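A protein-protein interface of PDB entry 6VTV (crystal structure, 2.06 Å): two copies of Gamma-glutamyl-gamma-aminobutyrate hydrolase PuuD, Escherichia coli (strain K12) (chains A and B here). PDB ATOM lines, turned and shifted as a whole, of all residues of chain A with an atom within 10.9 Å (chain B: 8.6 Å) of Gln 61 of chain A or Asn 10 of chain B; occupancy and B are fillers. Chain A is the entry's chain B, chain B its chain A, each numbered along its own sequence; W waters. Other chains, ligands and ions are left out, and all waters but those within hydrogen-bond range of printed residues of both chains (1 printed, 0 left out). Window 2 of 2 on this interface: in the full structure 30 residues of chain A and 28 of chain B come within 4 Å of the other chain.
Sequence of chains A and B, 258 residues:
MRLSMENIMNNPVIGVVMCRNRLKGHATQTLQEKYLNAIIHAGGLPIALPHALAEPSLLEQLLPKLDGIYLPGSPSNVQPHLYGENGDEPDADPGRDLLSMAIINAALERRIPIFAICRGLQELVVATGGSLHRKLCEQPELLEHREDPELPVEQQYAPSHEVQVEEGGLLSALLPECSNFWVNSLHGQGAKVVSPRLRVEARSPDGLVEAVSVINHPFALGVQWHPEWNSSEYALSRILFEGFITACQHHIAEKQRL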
ATOM      1  N   VAL A  13      -0.715  -1.112  12.935  1.00  0.00           N
ATOM      2  CA  VAL A  13      -0.099  -1.783  11.794  1.00  0.00           C
ATOM      3  C   VAL A  13      -0.327  -0.934  10.551  1.00  0.00           C
ATOM      4  O   VAL A  13      -1.471  -0.664  10.172  1.00  0.00           O
ATOM      5  CB  VAL A  13      -0.667  -3.197  11.606  1.00  0.00           C
ATOM      6  CG1 VAL A  13       0.007  -3.882  10.425  1.00  0.00           C
ATOM      7  CG2 VAL A  13      -0.498  -4.014  12.876  1.00  0.00           C
ATOM      8  N   ILE A  47       4.638  -2.579   7.845  1.00  0.00           N
ATOM      9  CA  ILE A  47       4.908  -3.818   7.128  1.00  0.00           C
ATOM     10  C   ILE A  47       4.808  -3.516   5.639  1.00  0.00           C
ATOM     11  O   ILE A  47       3.862  -2.855   5.196  1.00  0.00           O
ATOM     12  CB  ILE A  47       3.949  -4.954   7.534  1.00  0.00           C
ATOM     13  CG1 ILE A  47       2.488  -4.528   7.376  1.00  0.00           C
ATOM     14  CG2 ILE A  47       4.222  -5.397   8.966  1.00  0.00           C
ATOM     15  CD1 ILE A  47       1.512  -5.683   7.448  1.00  0.00           C
ATOM     16  N   LEU A  49       4.294  -4.157   1.678  1.00  0.00           N
ATOM     17  CA  LEU A  49       3.346  -4.965   0.921  1.00  0.00           C
ATOM     18  C   LEU A  49       3.849  -5.193  -0.497  1.00  0.00           C
ATOM     19  O   LEU A  49       3.914  -4.238  -1.287  1.00  0.00           O
ATOM     20  CB  LEU A  49       1.976  -4.285   0.894  1.00  0.00           C
ATOM     21  CG  LEU A  49       1.438  -3.813   2.246  1.00  0.00           C
ATOM     22  CD1 LEU A  49       0.144  -3.032   2.067  1.00  0.00           C
ATOM     23  CD2 LEU A  49       1.236  -4.989   3.189  1.00  0.00           C
ATOM     24  N   ALA A  52       2.430  -8.658  -5.386  1.00  0.00           N
ATOM     25  CA  ALA A  52       1.638  -9.874  -5.526  1.00  0.00           C
ATOM     26  C   ALA A  52       0.407  -9.866  -4.632  1.00  0.00           C
ATOM     27  O   ALA A  52      -0.553 -10.596  -4.906  1.00  0.00           O
ATOM     28  CB  ALA A  52       2.495 -11.103  -5.220  1.00  0.00           C
ATOM     29  N   LEU A  53       0.408  -9.054  -3.572  1.00  0.00           N
ATOM     30  CA  LEU A  53      -0.743  -8.956  -2.685  1.00  0.00           C
ATOM     31  C   LEU A  53      -1.934  -8.269  -3.337  1.00  0.00           C
ATOM     32  O   LEU A  53      -3.020  -8.265  -2.747  1.00  0.00           O
ATOM     33  CB  LEU A  53      -0.352  -8.215  -1.407  1.00  0.00           C
ATOM     34  CG  LEU A  53       0.716  -8.916  -0.569  1.00  0.00           C
ATOM     35  CD1 LEU A  53       0.896  -8.211   0.762  1.00  0.00           C
ATOM     36  CD2 LEU A  53       0.352 -10.378  -0.362  1.00  0.00           C
ATOM     37  N   ALA A  54      -1.760  -7.692  -4.529  1.00  0.00           N
ATOM     38  CA  ALA A  54      -2.886  -7.112  -5.249  1.00  0.00           C
ATOM     39  C   ALA A  54      -3.905  -8.165  -5.657  1.00  0.00           C
ATOM     40  O   ALA A  54      -5.022  -7.810  -6.050  1.00  0.00           O
ATOM     41  CB  ALA A  54      -2.392  -6.359  -6.484  1.00  0.00           C
ATOM     42  N   GLU A  55      -3.544  -9.441  -5.583  1.00  0.00           N
ATOM     43  CA  GLU A  55      -4.494 -10.509  -5.845  1.00  0.00           C
ATOM     44  C   GLU A  55      -5.676 -10.378  -4.886  1.00  0.00           C
ATOM     45  O   GLU A  55      -5.471 -10.260  -3.670  1.00  0.00           O
ATOM     46  CB  GLU A  55      -3.813 -11.869  -5.686  1.00  0.00           C
ATOM     47  CG  GLU A  55      -4.423 -12.986  -6.516  1.00  0.00           C
ATOM     48  CD  GLU A  55      -5.767 -13.432  -5.986  1.00  0.00           C
ATOM     49  OE1 GLU A  55      -5.909 -13.530  -4.750  1.00  0.00           O
ATOM     50  OE2 GLU A  55      -6.680 -13.683  -6.800  1.00  0.00           O
ATOM     51  N   PRO A  56      -6.916 -10.376  -5.389  1.00  0.00           N
ATOM     52  CA  PRO A  56      -8.061 -10.059  -4.517  1.00  0.00           C
ATOM     53  C   PRO A  56      -8.199 -10.967  -3.305  1.00  0.00           C
ATOM     54  O   PRO A  56      -8.494 -10.474  -2.209  1.00  0.00           O
ATOM     55  CB  PRO A  56      -9.259 -10.195  -5.466  1.00  0.00           C
ATOM     56  CG  PRO A  56      -8.695  -9.892  -6.815  1.00  0.00           C
ATOM     57  CD  PRO A  56      -7.306 -10.466  -6.807  1.00  0.00           C
ATOM     58  N   SER A  57      -7.995 -12.277  -3.462  1.00  0.00           N
ATOM     59  CA  SER A  57      -8.177 -13.180  -2.328  1.00  0.00           C
ATOM     60  C   SER A  57      -7.136 -12.939  -1.241  1.00  0.00           C
ATOM     61  O   SER A  57      -7.435 -13.104  -0.054  1.00  0.00           O
ATOM     62  CB  SER A  57      -8.134 -14.636  -2.794  1.00  0.00           C
ATOM     63  OG  SER A  57      -6.827 -15.013  -3.188  1.00  0.00           O
ATOM     64  N   LEU A  58      -5.919 -12.547  -1.621  1.00  0.00           N
ATOM     65  CA  LEU A  58      -4.901 -12.235  -0.623  1.00  0.00           C
ATOM     66  C   LEU A  58      -5.140 -10.869   0.011  1.00  0.00           C
ATOM     67  O   LEU A  58      -4.934 -10.698   1.217  1.00  0.00           O
ATOM     68  CB  LEU A  58      -3.509 -12.289  -1.253  1.00  0.00           C
ATOM     69  CG  LEU A  58      -3.092 -13.609  -1.900  1.00  0.00           C
ATOM     70  CD1 LEU A  58      -1.651 -13.528  -2.369  1.00  0.00           C
ATOM     71  CD2 LEU A  58      -3.278 -14.767  -0.932  1.00  0.00           C
ATOM     72  N   LEU A  59      -5.571  -9.889  -0.787  1.00  0.00           N
ATOM     73  CA  LEU A  59      -5.804  -8.550  -0.259  1.00  0.00           C
ATOM     74  C   LEU A  59      -6.930  -8.547   0.768  1.00  0.00           C
ATOM     75  O   LEU A  59      -6.826  -7.891   1.811  1.00  0.00           O
ATOM     76  CB  LEU A  59      -6.117  -7.584  -1.401  1.00  0.00           C
ATOM     77  CG  LEU A  59      -6.037  -6.091  -1.078  1.00  0.00           C
ATOM     78  CD1 LEU A  59      -4.606  -5.682  -0.776  1.00  0.00           C
ATOM     79  CD2 LEU A  59      -6.608  -5.264  -2.221  1.00  0.00           C
ATOM     80  N   GLU A  60      -8.015  -9.277   0.491  1.00  0.00           N
ATOM     81  CA  GLU A  60      -9.139  -9.317   1.422  1.00  0.00           C
ATOM     82  C   GLU A  60      -8.744  -9.932   2.758  1.00  0.00           C
ATOM     83  O   GLU A  60      -9.285  -9.548   3.802  1.00  0.00           O
ATOM     84  CB  GLU A  60     -10.304 -10.090   0.808  1.00  0.00           C
ATOM     85  CG  GLU A  60     -11.009  -9.362  -0.326  1.00  0.00           C
ATOM     86  CD  GLU A  60     -11.964  -8.294   0.170  1.00  0.00           C
ATOM     87  OE1 GLU A  60     -11.592  -7.102   0.138  1.00  0.00           O
ATOM     88  OE2 GLU A  60     -13.087  -8.645   0.590  1.00  0.00           O
ATOM     89  N   GLN A  61      -7.809 -10.885   2.751  1.00  0.00           N
ATOM     90  CA  GLN A  61      -7.367 -11.491   4.002  1.00  0.00           C
ATOM     91  C   GLN A  61      -6.472 -10.552   4.801  1.00  0.00           C
ATOM     92  O   GLN A  61      -6.441 -10.628   6.034  1.00  0.00           O
ATOM     93  CB  GLN A  61      -6.632 -12.801   3.722  1.00  0.00           C
ATOM     94  CG  GLN A  61      -7.513 -13.923   3.201  1.00  0.00           C
ATOM     95  CD  GLN A  61      -6.711 -15.150   2.813  1.00  0.00           C
ATOM     96  OE1 GLN A  61      -6.284 -15.921   3.672  1.00  0.00           O
ATOM     97  NE2 GLN A  61      -6.500 -15.334   1.516  1.00  0.00           N
ATOM     98  N   LEU A  62      -5.746  -9.663   4.124  1.00  0.00           N
ATOM     99  CA  LEU A  62      -4.768  -8.808   4.785  1.00  0.00           C
ATOM    100  C   LEU A  62      -5.386  -7.532   5.350  1.00  0.00           C
ATOM    101  O   LEU A  62      -4.972  -7.070   6.420  1.00  0.00           O
ATOM    102  CB  LEU A  62      -3.647  -8.446   3.806  1.00  0.00           C
ATOM    103  CG  LEU A  62      -2.495  -7.604   4.363  1.00  0.00           C
ATOM    104  CD1 LEU A  62      -2.016  -8.143   5.705  1.00  0.00           C
ATOM    105  CD2 LEU A  62      -1.356  -7.540   3.371  1.00  0.00           C
ATOM    106  N   LEU A  63      -6.364  -6.956   4.654  1.00  0.00           N
ATOM    107  CA  LEU A  63      -6.938  -5.677   5.067  1.00  0.00           C
ATOM    108  C   LEU A  63      -7.408  -5.629   6.519  1.00  0.00           C
ATOM    109  O   LEU A  63      -7.154  -4.607   7.180  1.00  0.00           O
ATOM    110  CB  LEU A  63      -8.090  -5.307   4.123  1.00  0.00           C
ATOM    111  CG  LEU A  63      -7.675  -4.920   2.703  1.00  0.00           C
ATOM    112  CD1 LEU A  63      -8.884  -4.942   1.792  1.00  0.00           C
ATOM    113  CD2 LEU A  63      -7.000  -3.554   2.681  1.00  0.00           C
ATOM    114  N   PRO A  64      -8.079  -6.647   7.075  1.00  0.00           N
ATOM    115  CA  PRO A  64      -8.472  -6.565   8.493  1.00  0.00           C
ATOM    116  C   PRO A  64      -7.301  -6.417   9.448  1.00  0.00           C
ATOM    117  O   PRO A  64      -7.499  -5.956  10.579  1.00  0.00           O
ATOM    118  CB  PRO A  64      -9.216  -7.886   8.730  1.00  0.00           C
ATOM    119  CG  PRO A  64      -9.704  -8.285   7.390  1.00  0.00           C
ATOM    120  CD  PRO A  64      -8.638  -7.851   6.434  1.00  0.00           C
ATOM    121  N   LYS A  65      -6.092  -6.787   9.035  1.00  0.00           N
ATOM    122  CA  LYS A  65      -4.914  -6.687   9.884  1.00  0.00           C
ATOM    123  C   LYS A  65      -4.166  -5.371   9.712  1.00  0.00           C
ATOM    124  O   LYS A  65      -3.171  -5.145  10.410  1.00  0.00           O
ATOM    125  CB  LYS A  65      -3.976  -7.866   9.607  1.00  0.00           C
ATOM    126  CG  LYS A  65      -4.551  -9.201  10.055  1.00  0.00           C
ATOM    127  CD  LYS A  65      -3.926 -10.372   9.316  1.00  0.00           C
ATOM    128  CE  LYS A  65      -4.516 -11.689   9.795  1.00  0.00           C
ATOM    129  NZ  LYS A  65      -4.147 -12.826   8.909  1.00  0.00           N
ATOM    130  N   LEU A  66      -4.619  -4.500   8.816  1.00  0.00           N
ATOM    131  CA  LEU A  66      -3.993  -3.205   8.592  1.00  0.00           C
ATOM    132  C   LEU A  66      -4.819  -2.113   9.258  1.00  0.00           C
ATOM    133  O   LEU A  66      -6.035  -2.030   9.047  1.00  0.00           O
ATOM    134  CB  LEU A  66      -3.852  -2.917   7.097  1.00  0.00           C
ATOM    135  CG  LEU A  66      -3.077  -3.950   6.279  1.00  0.00           C
ATOM    136  CD1 LEU A  66      -3.170  -3.636   4.795  1.00  0.00           C
ATOM    137  CD2 LEU A  66      -1.627  -3.999   6.729  1.00  0.00           C
ATOM    138  N   ASP A  67      -4.160  -1.282  10.063  1.00  0.00           N
ATOM    139  CA  ASP A  67      -4.800  -0.126  10.672  1.00  0.00           C
ATOM    140  C   ASP A  67      -4.601   1.151   9.867  1.00  0.00           C
ATOM    141  O   ASP A  67      -5.207   2.174  10.198  1.00  0.00           O
ATOM    142  CB  ASP A  67      -4.277   0.082  12.100  1.00  0.00           C
ATOM    143  CG  ASP A  67      -4.339  -1.185  12.934  1.00  0.00           C
ATOM    144  OD1 ASP A  67      -5.417  -1.815  12.988  1.00  0.00           O
ATOM    145  OD2 ASP A  67      -3.308  -1.550  13.537  1.00  0.00           O
ATOM    146  N   ILE A  69      -2.986   2.672   5.688  1.00  0.00           N
ATOM    147  CA  ILE A  69      -2.353   2.446   4.393  1.00  0.00           C
ATOM    148  C   ILE A  69      -1.392   3.596   4.122  1.00  0.00           C
ATOM    149  O   ILE A  69      -1.749   4.766   4.301  1.00  0.00           O
ATOM    150  CB  ILE A  69      -3.389   2.318   3.262  1.00  0.00           C
ATOM    151  CG1 ILE A  69      -4.389   1.202   3.576  1.00  0.00           C
ATOM    152  CG2 ILE A  69      -2.699   2.049   1.933  1.00  0.00           C
ATOM    153  CD1 ILE A  69      -3.740  -0.125   3.901  1.00  0.00           C
ATOM    154  N   ILE A 103      -5.744  -1.278  -3.330  1.00  0.00           N
ATOM    155  CA  ILE A 103      -5.745  -1.060  -1.888  1.00  0.00           C
ATOM    156  C   ILE A 103      -6.356   0.293  -1.526  1.00  0.00           C
ATOM    157  O   ILE A 103      -6.889   0.455  -0.422  1.00  0.00           O
ATOM    158  CB  ILE A 103      -4.323  -1.219  -1.321  1.00  0.00           C
ATOM    159  CG1 ILE A 103      -4.385  -1.558   0.170  1.00  0.00           C
ATOM    160  CG2 ILE A 103      -3.489   0.032  -1.563  1.00  0.00           C
ATOM    161  CD1 ILE A 103      -3.126  -2.197   0.701  1.00  0.00           C
ATOM    162  N   ALA A 106     -10.208  -0.332  -1.710  1.00  0.00           N
ATOM    163  CA  ALA A 106     -10.612  -1.153  -0.575  1.00  0.00           C
ATOM    164  C   ALA A 106     -10.572  -0.359   0.725  1.00  0.00           C
ATOM    165  O   ALA A 106     -11.490  -0.457   1.546  1.00  0.00           O
ATOM    166  CB  ALA A 106      -9.718  -2.387  -0.483  1.00  0.00           C
ATOM    167  N   ARG A 110     -13.620   0.547   3.427  1.00  0.00           N
ATOM    168  CA  ARG A 110     -13.455   0.123   4.812  1.00  0.00           C
ATOM    169  C   ARG A 110     -13.111   1.272   5.751  1.00  0.00           C
ATOM    170  O   ARG A 110     -12.941   1.036   6.952  1.00  0.00           O
ATOM    171  CB  ARG A 110     -12.370  -0.955   4.905  1.00  0.00           C
ATOM    172  CG  ARG A 110     -12.608  -2.146   3.994  1.00  0.00           C
ATOM    173  CD  ARG A 110     -11.631  -3.272   4.275  1.00  0.00           C
ATOM    174  NE  ARG A 110     -11.944  -4.461   3.488  1.00  0.00           N
ATOM    175  CZ  ARG A 110     -11.916  -5.699   3.966  1.00  0.00           C
ATOM    176  NH1 ARG A 110     -11.589  -5.912   5.233  1.00  0.00           N
ATOM    177  NH2 ARG A 110     -12.215  -6.725   3.180  1.00  0.00           N
ATOM    178  N   ILE A 112     -10.412   2.828   6.148  1.00  0.00           N
ATOM    179  CA  ILE A 112      -9.066   2.683   6.707  1.00  0.00           C
ATOM    180  C   ILE A 112      -8.270   3.948   6.397  1.00  0.00           C
ATOM    181  O   ILE A 112      -8.289   4.412   5.247  1.00  0.00           O
ATOM    182  CB  ILE A 112      -8.377   1.448   6.131  1.00  0.00           C
ATOM    183  CG1 ILE A 112      -9.189   0.188   6.438  1.00  0.00           C
ATOM    184  CG2 ILE A 112      -6.960   1.319   6.674  1.00  0.00           C
ATOM    185  CD1 ILE A 112      -8.686  -1.045   5.718  1.00  0.00           C
ATOM    186  N   LYS A 255     -13.116   0.599  15.278  1.00  0.00           N
ATOM    187  CA  LYS A 255     -13.346  -0.789  14.895  1.00  0.00           C
ATOM    188  C   LYS A 255     -14.043  -1.599  15.976  1.00  0.00           C
ATOM    189  O   LYS A 255     -14.242  -2.805  15.793  1.00  0.00           O
ATOM    190  CB  LYS A 255     -12.023  -1.460  14.521  1.00  0.00           C
ATOM    191  CG  LYS A 255     -11.875  -1.688  13.036  1.00  0.00           C
ATOM    192  CD  LYS A 255     -10.731  -2.627  12.713  1.00  0.00           C
ATOM    193  CE  LYS A 255      -9.380  -1.985  12.987  1.00  0.00           C
ATOM    194  NZ  LYS A 255      -8.313  -2.609  12.157  1.00  0.00           N
ATOM    195  N   ASN B  10      -7.748 -20.348   3.842  1.00  0.00           N
ATOM    196  CA  ASN B  10      -7.002 -19.148   4.201  1.00  0.00           C
ATOM    197  C   ASN B  10      -5.503 -19.367   4.034  1.00  0.00           C
ATOM    198  O   ASN B  10      -4.990 -20.454   4.295  1.00  0.00           O
ATOM    199  CB  ASN B  10      -7.316 -18.728   5.638  1.00  0.00           C
ATOM    200  CG  ASN B  10      -8.803 -18.695   5.922  1.00  0.00           C
ATOM    201  OD1 ASN B  10      -9.232 -18.293   7.005  1.00  0.00           O
ATOM    202  ND2 ASN B  10      -9.601 -19.119   4.948  1.00  0.00           N
ATOM    203  N   ASN B  11      -4.800 -18.322   3.600  1.00  0.00           N
ATOM    204  CA  ASN B  11      -3.373 -18.414   3.344  1.00  0.00           C
ATOM    205  C   ASN B  11      -2.602 -17.897   4.547  1.00  0.00           C
ATOM    206  O   ASN B  11      -2.817 -16.745   4.956  1.00  0.00           O
ATOM    207  CB  ASN B  11      -3.004 -17.620   2.096  1.00  0.00           C
ATOM    208  CG  ASN B  11      -3.795 -18.055   0.873  1.00  0.00           C
ATOM    209  OD1 ASN B  11      -4.954 -17.675   0.700  1.00  0.00           O
ATOM    210  ND2 ASN B  11      -3.170 -18.859   0.020  1.00  0.00           N
ATOM    211  N   PRO B  12      -1.713 -18.694   5.141  1.00  0.00           N
ATOM    212  CA  PRO B  12      -0.977 -18.224   6.321  1.00  0.00           C
ATOM    213  C   PRO B  12      -0.100 -17.023   5.991  1.00  0.00           C
ATOM    214  O   PRO B  12       0.496 -16.942   4.915  1.00  0.00           O
ATOM    215  CB  PRO B  12      -0.136 -19.441   6.729  1.00  0.00           C
ATOM    216  CG  PRO B  12      -0.094 -20.316   5.521  1.00  0.00           C
ATOM    217  CD  PRO B  12      -1.381 -20.085   4.793  1.00  0.00           C
ATOM    218  N   VAL B  13      -0.034 -16.087   6.934  1.00  0.00           N
ATOM    219  CA  VAL B  13       0.753 -14.869   6.770  1.00  0.00           C
ATOM    220  C   VAL B  13       2.217 -15.196   7.033  1.00  0.00           C
ATOM    221  O   VAL B  13       2.566 -15.701   8.105  1.00  0.00           O
ATOM    222  CB  VAL B  13       0.253 -13.763   7.709  1.00  0.00           C
ATOM    223  CG1 VAL B  13       1.065 -12.489   7.514  1.00  0.00           C
ATOM    224  CG2 VAL B  13      -1.227 -13.506   7.475  1.00  0.00           C
ATOM    225  N   ALA B  42       3.171 -21.657  -3.129  1.00  0.00           N
ATOM    226  CA  ALA B  42       2.942 -22.677  -2.115  1.00  0.00           C
ATOM    227  C   ALA B  42       1.719 -22.396  -1.251  1.00  0.00           C
ATOM    228  O   ALA B  42       1.348 -23.250  -0.437  1.00  0.00           O
ATOM    229  CB  ALA B  42       4.177 -22.824  -1.226  1.00  0.00           C
ATOM    230  N   GLY B  43       1.090 -21.236  -1.400  1.00  0.00           N
ATOM    231  CA  GLY B  43      -0.118 -20.922  -0.669  1.00  0.00           C
ATOM    232  C   GLY B  43       0.034 -19.976   0.502  1.00  0.00           C
ATOM    233  O   GLY B  43      -0.866 -19.921   1.346  1.00  0.00           O
ATOM    234  N   GLY B  44       1.134 -19.229   0.580  1.00  0.00           N
ATOM    235  CA  GLY B  44       1.352 -18.302   1.667  1.00  0.00           C
ATOM    236  C   GLY B  44       1.041 -16.866   1.287  1.00  0.00           C
ATOM    237  O   GLY B  44       1.027 -16.499   0.114  1.00  0.00           O
ATOM    238  N   LEU B  45       0.778 -16.052   2.310  1.00  0.00           N
ATOM    239  CA  LEU B  45       0.548 -14.620   2.142  1.00  0.00           C
ATOM    240  C   LEU B  45       1.759 -13.865   2.671  1.00  0.00           C
ATOM    241  O   LEU B  45       1.886 -13.673   3.890  1.00  0.00           O
ATOM    242  CB  LEU B  45      -0.724 -14.180   2.874  1.00  0.00           C
ATOM    243  CG  LEU B  45      -1.351 -12.855   2.430  1.00  0.00           C
ATOM    244  CD1 LEU B  45      -2.856 -12.888   2.640  1.00  0.00           C
ATOM    245  CD2 LEU B  45      -0.736 -11.671   3.169  1.00  0.00           C
ATOM    246  N   ASP B  67       2.219 -16.214  10.932  1.00  0.00           N
ATOM    247  CA  ASP B  67       2.080 -17.658  10.998  1.00  0.00           C
ATOM    248  C   ASP B  67       3.367 -18.390  10.644  1.00  0.00           C
ATOM    249  O   ASP B  67       3.469 -19.593  10.909  1.00  0.00           O
ATOM    250  CB  ASP B  67       0.943 -18.119  10.075  1.00  0.00           C
ATOM    251  CG  ASP B  67      -0.363 -17.395  10.358  1.00  0.00           C
ATOM    252  OD1 ASP B  67      -0.706 -17.232  11.548  1.00  0.00           O
ATOM    253  OD2 ASP B  67      -1.045 -16.984   9.395  1.00  0.00           O
ATOM    254  N   ILE B 245       4.583 -24.380   4.410  1.00  0.00           N
ATOM    255  CA  ILE B 245       3.228 -23.839   4.508  1.00  0.00           C
ATOM    256  C   ILE B 245       2.345 -24.751   5.354  1.00  0.00           C
ATOM    257  O   ILE B 245       1.543 -24.277   6.170  1.00  0.00           O
ATOM    258  CB  ILE B 245       2.640 -23.618   3.103  1.00  0.00           C
ATOM    259  CG1 ILE B 245       3.481 -22.603   2.327  1.00  0.00           C
ATOM    260  CG2 ILE B 245       1.196 -23.156   3.190  1.00  0.00           C
ATOM    261  CD1 ILE B 245       3.529 -21.231   2.968  1.00  0.00           C
ATOM    262  N   CYS B 248       2.932 -24.057   8.852  1.00  0.00           N
ATOM    263  CA  CYS B 248       2.302 -22.804   9.253  1.00  0.00           C
ATOM    264  C   CYS B 248       0.811 -22.978   9.495  1.00  0.00           C
ATOM    265  O   CYS B 248       0.235 -22.296  10.353  1.00  0.00           O
ATOM    266  CB  CYS B 248       2.517 -21.749   8.171  1.00  0.00           C
ATOM    267  SG  CYS B 248       4.224 -21.162   7.978  1.00  0.00           S
ATOM    268  N   GLN B 249       0.167 -23.861   8.725  1.00  0.00           N
ATOM    269  CA  GLN B 249      -1.246 -24.140   8.937  1.00  0.00           C
ATOM    270  C   GLN B 249      -1.466 -24.855  10.260  1.00  0.00           C
ATOM    271  O   GLN B 249      -2.461 -24.604  10.948  1.00  0.00           O
ATOM    272  CB  GLN B 249      -1.798 -24.969   7.778  1.00  0.00           C
ATOM    273  CG  GLN B 249      -1.923 -24.208   6.464  1.00  0.00           C
ATOM    274  CD  GLN B 249      -2.220 -25.115   5.285  1.00  0.00           C
ATOM    275  OE1 GLN B 249      -1.626 -26.183   5.144  1.00  0.00           O
ATOM    276  NE2 GLN B 249      -3.144 -24.690   4.428  1.00  0.00           N
ATOM    277  N   ILE B 252      -1.414 -22.251  12.821  1.00  0.00           N
ATOM    278  CA  ILE B 252      -2.661 -21.493  12.866  1.00  0.00           C
ATOM    279  C   ILE B 252      -3.696 -22.225  13.712  1.00  0.00           C
ATOM    280  O   ILE B 252      -4.347 -21.630  14.579  1.00  0.00           O
ATOM    281  CB  ILE B 252      -3.182 -21.231  11.441  1.00  0.00           C
ATOM    282  CG1 ILE B 252      -2.256 -20.264  10.702  1.00  0.00           C
ATOM    283  CG2 ILE B 252      -4.598 -20.681  11.481  1.00  0.00           C
ATOM    284  CD1 ILE B 252      -2.680 -19.995   9.277  1.00  0.00           C
ATOM    285  N   GLN B 256      -5.584 -21.044  17.318  1.00  0.00           N
ATOM    286  CA  GLN B 256      -7.033 -20.991  17.450  1.00  0.00           C
ATOM    287  C   GLN B 256      -7.561 -21.930  18.527  1.00  0.00           C
ATOM    288  O   GLN B 256      -8.702 -21.762  18.971  1.00  0.00           O
ATOM    289  CB  GLN B 256      -7.695 -21.321  16.109  1.00  0.00           C
ATOM    290  CG  GLN B 256      -7.352 -20.345  14.993  1.00  0.00           C
ATOM    291  CD  GLN B 256      -7.781 -20.845  13.626  1.00  0.00           C
ATOM    292  OE1 GLN B 256      -8.009 -22.039  13.432  1.00  0.00           O
ATOM    293  NE2 GLN B 256      -7.890 -19.931  12.669  1.00  0.00           N
HETATM  294  O   HOH W   1      -4.504 -14.783   5.850  1.00  0.00           O
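The backbone NH of Asn 11 of chain B lies within hydrogen-bond range of the side-chain amide oxygen of Gln 61 of chain A (2.8 Å).
The backbone carbonyl oxygen of Gly 43 of chain B sits at hydrogen-bond distance from the side-chain amide nitrogen of Asn 11 of chain B (2.9 Å). The backbone NH (N) of Leu 45 of chain B is in hydrogen-bond range of the backbone carbonyl oxygen (O) of Pro 12 of chain B, at 2.8 Å. N of Val 13 of chain B sits at hydrogen-bond distance from OD2 of Asp 67 of chain B, 2.8 Å away. OE1 of Glu 55 of chain A sits at hydrogen-bond distance from N of Leu 58 of chain A (3.3 Å). The side-chain amide nitrogen of Gln 61 of chain A sits at hydrogen-bond distance from the backbone carbonyl oxygen of Ser 57 of chain A, at 2.9 Å.
CD2 of Leu 53 of chain A touches CD2 of Leu 45 of chain B, at 3.9 Å. Asn 11 of chain B touches Leu 58 of chain A (OD1 to CD2, 3.7 Å). Leu 45 of chain B touches Leu 58 of chain A (CD1 to O, 3.3 Å). Gln 61 of chain A touches Asn 10 of chain B (OE1 to CA, 3.3 Å). Gln 61 of chain A touches Leu 45 of chain B (CB to CD1, 3.9 Å). NZ of Lys 65 of chain A touches CG2 of Val 13 of chain B, 3.3 Å away.
Of the printed residues of chain B, Leu 53 of chain A touches Leu 45 (3.9 Å). Printed residues of chain B within 4 Å of Leu 58 of chain A: Asn 11 (3.7 Å) and Leu 45 (3.3 Å). Of chain B, only Asn 10 (3.3 Å), Asn 11 (2.8 Å) and Leu 45 (3.9 Å) come within 4 Å of Gln 61 of chain A. Leu 63 of chain A touches none of the printed residues of chain B. Printed residues of chain B within 4 Å of Lys 65 of chain A: Val 13. Lys 255 of chain A touches none of the printed residues of chain B. Of the printed residues of chain A, Val 13 of chain B touches Lys 65 (3.3 Å). The nearest residue of chain A that does not touch Asn 10 of chain B is Leu 58 of chain A (7.1 Å).
Along chain A the printed residues that touch a printed residue of chain B span positions 53 to 65. Along chain B the printed residues that touch a printed residue of chain A span positions 10 to 45. Among the printed residues, no Asp or Glu carboxylate lies within 4 Å of a Lys or Arg side-chain nitrogen of the other chain.
2 positions are printed for both chains. Of the 7 pairs that touch across the chains among the printed residues, none has its exchanged pair printed and touching as well.
Water W1 bridges O of Asn 11 of chain B and OE1 of Gln 61 of chain A.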
